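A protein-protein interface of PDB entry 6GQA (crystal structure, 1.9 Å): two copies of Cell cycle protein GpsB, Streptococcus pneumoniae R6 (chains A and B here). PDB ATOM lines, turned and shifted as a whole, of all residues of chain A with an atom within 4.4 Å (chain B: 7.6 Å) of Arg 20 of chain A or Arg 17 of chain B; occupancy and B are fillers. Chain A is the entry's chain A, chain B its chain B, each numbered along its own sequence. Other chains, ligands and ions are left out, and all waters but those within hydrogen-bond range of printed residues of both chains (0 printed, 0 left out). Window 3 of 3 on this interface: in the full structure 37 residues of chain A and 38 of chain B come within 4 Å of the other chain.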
ATOM      1  N   GLU A  18     -23.607 -29.529  19.330  1.00  0.00           N
ATOM      2  CA  GLU A  18     -24.434 -30.734  19.293  1.00  0.00           C
ATOM      3  C   GLU A  18     -25.631 -30.455  18.405  1.00  0.00           C
ATOM      4  O   GLU A  18     -25.902 -29.309  18.064  1.00  0.00           O
ATOM      5  CB  GLU A  18     -24.913 -31.131  20.678  1.00  0.00           C
ATOM      6  CG  GLU A  18     -25.907 -30.104  21.204  1.00  0.00           C
ATOM      7  CD  GLU A  18     -26.512 -30.512  22.519  1.00  0.00           C
ATOM      8  OE1 GLU A  18     -27.023 -31.619  22.659  1.00  0.00           O
ATOM      9  OE2 GLU A  18     -26.453 -29.734  23.448  1.00  0.00           O
ATOM     10  N   VAL A  19     -26.394 -31.508  18.087  1.00  0.00           N
ATOM     11  CA  VAL A  19     -27.445 -31.353  17.098  1.00  0.00           C
ATOM     12  C   VAL A  19     -28.577 -30.481  17.635  1.00  0.00           C
ATOM     13  O   VAL A  19     -29.110 -29.631  16.911  1.00  0.00           O
ATOM     14  CB  VAL A  19     -27.956 -32.731  16.611  1.00  0.00           C
ATOM     15  CG1 VAL A  19     -28.380 -33.583  17.758  1.00  0.00           C
ATOM     16  CG2 VAL A  19     -29.117 -32.544  15.700  1.00  0.00           C
ATOM     17  N   ARG A  20     -28.989 -30.685  18.890  1.00  0.00           N
ATOM     18  CA  ARG A  20     -29.989 -29.844  19.540  1.00  0.00           C
ATOM     19  C   ARG A  20     -29.330 -28.735  20.351  1.00  0.00           C
ATOM     20  O   ARG A  20     -29.540 -28.593  21.546  1.00  0.00           O
ATOM     21  CB  ARG A  20     -30.872 -30.690  20.434  1.00  0.00           C
ATOM     22  CG  ARG A  20     -31.707 -31.757  19.705  1.00  0.00           C
ATOM     23  CD  ARG A  20     -32.751 -32.232  20.679  1.00  0.00           C
ATOM     24  NE  ARG A  20     -33.593 -33.327  20.208  1.00  0.00           N
ATOM     25  CZ  ARG A  20     -33.098 -34.510  19.869  1.00  0.00           C
ATOM     26  NH1 ARG A  20     -31.784 -34.722  19.951  1.00  0.00           N
ATOM     27  NH2 ARG A  20     -33.890 -35.478  19.442  1.00  0.00           N
ATOM     28  N   GLY A  21     -28.513 -27.942  19.693  1.00  0.00           N
ATOM     29  CA  GLY A  21     -27.733 -26.947  20.408  1.00  0.00           C
ATOM     30  C   GLY A  21     -28.460 -25.626  20.698  1.00  0.00           C
ATOM     31  O   GLY A  21     -29.637 -25.436  20.373  1.00  0.00           O
ATOM     32  N   TYR A  22     -27.713 -24.705  21.345  1.00  0.00           N
ATOM     33  CA  TYR A  22     -28.139 -23.328  21.560  1.00  0.00           C
ATOM     34  C   TYR A  22     -27.693 -22.421  20.405  1.00  0.00           C
ATOM     35  O   TYR A  22     -26.566 -22.529  19.894  1.00  0.00           O
ATOM     36  CB  TYR A  22     -27.550 -22.778  22.875  1.00  0.00           C
ATOM     37  CG  TYR A  22     -28.041 -23.329  24.189  1.00  0.00           C
ATOM     38  CD1 TYR A  22     -29.384 -23.640  24.401  1.00  0.00           C
ATOM     39  CD2 TYR A  22     -27.160 -23.497  25.246  1.00  0.00           C
ATOM     40  CE1 TYR A  22     -29.831 -24.141  25.664  1.00  0.00           C
ATOM     41  CE2 TYR A  22     -27.581 -23.986  26.505  1.00  0.00           C
ATOM     42  CZ  TYR A  22     -28.908 -24.308  26.686  1.00  0.00           C
ATOM     43  OH  TYR A  22     -29.277 -24.756  27.914  1.00  0.00           O
ATOM     44  N   PHE B  15     -31.890 -19.828  25.643  1.00  0.00           N
ATOM     45  CA  PHE B  15     -31.403 -19.660  24.279  1.00  0.00           C
ATOM     46  C   PHE B  15     -32.267 -20.507  23.360  1.00  0.00           C
ATOM     47  O   PHE B  15     -32.746 -21.565  23.771  1.00  0.00           O
ATOM     48  CB  PHE B  15     -29.935 -20.080  24.143  1.00  0.00           C
ATOM     49  CG  PHE B  15     -29.021 -19.328  25.088  1.00  0.00           C
ATOM     50  CD1 PHE B  15     -28.784 -17.962  24.886  1.00  0.00           C
ATOM     51  CD2 PHE B  15     -28.415 -19.971  26.163  1.00  0.00           C
ATOM     52  CE1 PHE B  15     -27.987 -17.204  25.758  1.00  0.00           C
ATOM     53  CE2 PHE B  15     -27.549 -19.252  27.009  1.00  0.00           C
ATOM     54  CZ  PHE B  15     -27.358 -17.838  26.787  1.00  0.00           C
ATOM     55  N   GLY B  16     -32.462 -20.039  22.147  1.00  0.00           N
ATOM     56  CA  GLY B  16     -33.298 -20.761  21.205  1.00  0.00           C
ATOM     57  C   GLY B  16     -32.547 -21.951  20.641  1.00  0.00           C
ATOM     58  O   GLY B  16     -31.338 -22.089  20.813  1.00  0.00           O
ATOM     59  N   ARG B  17     -33.264 -22.841  19.956  1.00  0.00           N
ATOM     60  CA  ARG B  17     -32.587 -24.035  19.461  1.00  0.00           C
ATOM     61  C   ARG B  17     -31.919 -23.728  18.140  1.00  0.00           C
ATOM     62  O   ARG B  17     -32.460 -22.992  17.314  1.00  0.00           O
ATOM     63  CB  ARG B  17     -33.505 -25.240  19.250  1.00  0.00           C
ATOM     64  CG  ARG B  17     -32.569 -26.469  19.063  1.00  0.00           C
ATOM     65  CD  ARG B  17     -33.181 -27.629  18.531  1.00  0.00           C
ATOM     66  NE  ARG B  17     -33.968 -28.312  19.517  1.00  0.00           N
ATOM     67  CZ  ARG B  17     -34.688 -29.353  19.171  1.00  0.00           C
ATOM     68  NH1 ARG B  17     -34.612 -29.748  17.912  1.00  0.00           N
ATOM     69  NH2 ARG B  17     -35.437 -30.016  20.058  1.00  0.00           N
ATOM     70  N   GLU B  18     -30.749 -24.322  17.940  1.00  0.00           N
ATOM     71  CA  GLU B  18     -30.049 -24.207  16.681  1.00  0.00           C
ATOM     72  C   GLU B  18     -29.408 -25.540  16.426  1.00  0.00           C
ATOM     73  O   GLU B  18     -28.758 -26.105  17.306  1.00  0.00           O
ATOM     74  CB  GLU B  18     -28.966 -23.123  16.672  1.00  0.00           C
ATOM     75  CG  GLU B  18     -28.012 -23.297  15.498  1.00  0.00           C
ATOM     76  CD  GLU B  18     -27.174 -22.077  15.271  1.00  0.00           C
ATOM     77  OE1 GLU B  18     -26.717 -21.539  16.281  1.00  0.00           O
ATOM     78  OE2 GLU B  18     -26.966 -21.665  14.098  1.00  0.00           O
ATOM     79  N   VAL B  19     -29.603 -26.033  15.218  1.00  0.00           N
ATOM     80  CA  VAL B  19     -29.022 -27.316  14.873  1.00  0.00           C
ATOM     81  C   VAL B  19     -27.528 -27.125  14.733  1.00  0.00           C
ATOM     82  O   VAL B  19     -27.089 -26.267  13.971  1.00  0.00           O
ATOM     83  CB  VAL B  19     -29.632 -27.856  13.575  1.00  0.00           C
ATOM     84  CG1 VAL B  19     -28.735 -28.922  13.036  1.00  0.00           C
ATOM     85  CG2 VAL B  19     -31.032 -28.386  13.858  1.00  0.00           C
ATOM     86  N   ARG B  20     -26.750 -27.940  15.441  1.00  0.00           N
ATOM     87  CA  ARG B  20     -25.299 -27.807  15.557  1.00  0.00           C
ATOM     88  C   ARG B  20     -24.890 -26.510  16.242  1.00  0.00           C
ATOM     89  O   ARG B  20     -23.789 -26.030  16.047  1.00  0.00           O
ATOM     90  CB  ARG B  20     -24.591 -27.948  14.203  1.00  0.00           C
ATOM     91  CG  ARG B  20     -24.240 -29.368  13.873  1.00  0.00           C
ATOM     92  CD  ARG B  20     -23.547 -29.484  12.530  1.00  0.00           C
ATOM     93  NE  ARG B  20     -23.835 -30.744  11.879  1.00  0.00           N
ATOM     94  CZ  ARG B  20     -24.974 -31.008  11.244  1.00  0.00           C
ATOM     95  NH1 ARG B  20     -25.926 -30.083  11.197  1.00  0.00           N
ATOM     96  NH2 ARG B  20     -25.161 -32.192  10.659  1.00  0.00           N
ATOM     97  N   GLY B  21     -25.758 -25.953  17.079  1.00  0.00           N
ATOM     98  CA  GLY B  21     -25.373 -24.865  17.938  1.00  0.00           C
ATOM     99  C   GLY B  21     -24.514 -25.364  19.082  1.00  0.00           C
ATOM    100  O   GLY B  21     -24.030 -26.498  19.096  1.00  0.00           O
ATOM    101  N   TYR B  22     -24.306 -24.493  20.058  1.00  0.00           N
ATOM    102  CA  TYR B  22     -23.376 -24.837  21.122  1.00  0.00           C
ATOM    103  C   TYR B  22     -23.931 -25.954  21.981  1.00  0.00           C
ATOM    104  O   TYR B  22     -25.117 -26.003  22.243  1.00  0.00           O
ATOM    105  CB  TYR B  22     -23.103 -23.639  22.025  1.00  0.00           C
ATOM    106  CG  TYR B  22     -22.322 -22.517  21.383  1.00  0.00           C
ATOM    107  CD1 TYR B  22     -21.278 -22.768  20.521  1.00  0.00           C
ATOM    108  CD2 TYR B  22     -22.629 -21.197  21.683  1.00  0.00           C
ATOM    109  CE1 TYR B  22     -20.558 -21.714  19.959  1.00  0.00           C
ATOM    110  CE2 TYR B  22     -21.893 -20.129  21.143  1.00  0.00           C
ATOM    111  CZ  TYR B  22     -20.878 -20.406  20.279  1.00  0.00           C
ATOM    112  OH  TYR B  22     -20.171 -19.379  19.718  1.00  0.00           O
ATOM    113  N   ASN B  23     -23.035 -26.828  22.447  1.00  0.00           N
ATOM    114  CA  ASN B  23     -23.375 -27.871  23.395  1.00  0.00           C
ATOM    115  C   ASN B  23     -24.037 -27.272  24.640  1.00  0.00           C
ATOM    116  O   ASN B  23     -23.525 -26.319  25.249  1.00  0.00           O
ATOM    117  CB  ASN B  23     -22.096 -28.620  23.739  1.00  0.00           C
ATOM    118  CG  ASN B  23     -22.339 -29.758  24.638  1.00  0.00           C
ATOM    119  OD1 ASN B  23     -22.504 -29.581  25.832  1.00  0.00           O
ATOM    120  ND2 ASN B  23     -22.357 -30.949  24.093  1.00  0.00           N
ATOM    121  N   LYS B  24     -25.224 -27.774  24.962  1.00  0.00           N
ATOM    122  CA  LYS B  24     -26.026 -27.143  26.011  1.00  0.00           C
ATOM    123  C   LYS B  24     -25.379 -27.351  27.368  1.00  0.00           C
ATOM    124  O   LYS B  24     -25.288 -26.424  28.169  1.00  0.00           O
ATOM    125  CB  LYS B  24     -27.451 -27.728  25.996  1.00  0.00           C
ATOM    126  CG  LYS B  24     -28.282 -27.430  24.713  1.00  0.00           C
ATOM    127  CD  LYS B  24     -29.676 -27.830  24.816  1.00  0.00           C
ATOM    128  CE  LYS B  24     -29.797 -29.386  24.726  1.00  0.00           C
ATOM    129  NZ  LYS B  24     -30.647 -29.825  23.606  1.00  0.00           N
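O of Arg 20 of chain A is in hydrogen-bond range of NZ of Lys 24 of chain B (2.6 Å). The backbone carbonyl oxygen of Gly 21 of chain A sits at hydrogen-bond distance from the backbone NH of Glu 18 of chain B. N of Lys 24 of chain B lies within hydrogen-bond range of OE2 of Glu 18 of chain A (2.8 Å). The backbone NH (N) of Tyr 22 of chain B is in hydrogen-bond range of the backbone carbonyl oxygen (O) of Tyr 22 of chain A (3.0 Å). The backbone NH of Arg 20 of chain B lies close to the backbone carbonyl oxygen of Glu 18 of chain A (3.1 Å). N of Glu 18 of chain A is in hydrogen-bond range of O of Gly 21 of chain B. O of Val 19 of chain A lies within hydrogen-bond range of N of Arg 20 of chain B (3.3 Å).
Of the printed residues of chain B, Val 19 of chain A touches Glu 18, Val 19 and Arg 20. Of chain B, only Arg 17 (3.5 Å) and Lys 24 (2.6 Å) come within 4 Å of Arg 20 of chain A. Of the printed residues of chain B, Gly 21 of chain A touches Gly 16 (3.8 Å), Arg 17 (3.4 Å), Glu 18 (2.9 Å), Gly 21 (3.8 Å) and Tyr 22 (3.3 Å). Of the printed residues of chain A, Gly 16 of chain B touches Gly 21 (3.8 Å) and Tyr 22 (3.5 Å). Arg 17 of chain B touches two residues of chain A. Printed residues of chain A within 4 Å of Val 19 of chain B: Val 19 (3.1 Å). The nearest printed residue of chain B that does not touch Tyr 22 of chain A is Asn 23 of chain B (4.6 Å).
Among the printed residues, pairs that only touch across the chains: Val 19 of chain A with Val 19 of chain B, Tyr 22 of chain A with Gly 21 of chain B, Gly 21 of chain A with Tyr 22 of chain B, Gly 21 of chain A with Arg 17 of chain B, Tyr 22 of chain A with Gly 16 of chain B, Arg 20 of chain A with Arg 17 of chain B, Tyr 22 of chain A with Lys 24 of chain B, Val 19 of chain A with Glu 18 of chain B, Glu 18 of chain A with Asn 23 of chain B, Tyr 22 of chain A with Phe 15 of chain B, Tyr 22 of chain A with Glu 18 of chain B, Gly 21 of chain A with Gly 16 of chain B and Gly 21 of chain A with Gly 21 of chain B.
Of the 10 printed residues of chain B, 10 touch a printed residue of chain A. Hydrophobic or aromatic side chains of chain B that line the printed part of chain A: Phe 15 and Val 19. Printed residues of chain A that touch a printed residue of chain B: Glu 18, Val 19, Arg 20, Gly 21 and Tyr 22. Hydrophobic or aromatic side chains of chain A that line the printed part of chain B: Tyr 22.
Glu 18 of chain A touches Gly 21 of chain B, and with the chains exchanged Gly 21 of chain A touches Glu 18 of chain B. Val 19 of chain A touches Arg 20 of chain B, but with the chains exchanged Arg 20 of chain A does not touch Val 19 of chain B (5.2 Å). Gly 21 of chain A touches its own counterpart, Gly 21 of chain B. Tyr 22 of chain A touches its own counterpart, Tyr 22 of chain B. Of the 20 pairs that touch across the chains among the printed residues, 7 have their exchanged pair printed and touching as well.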
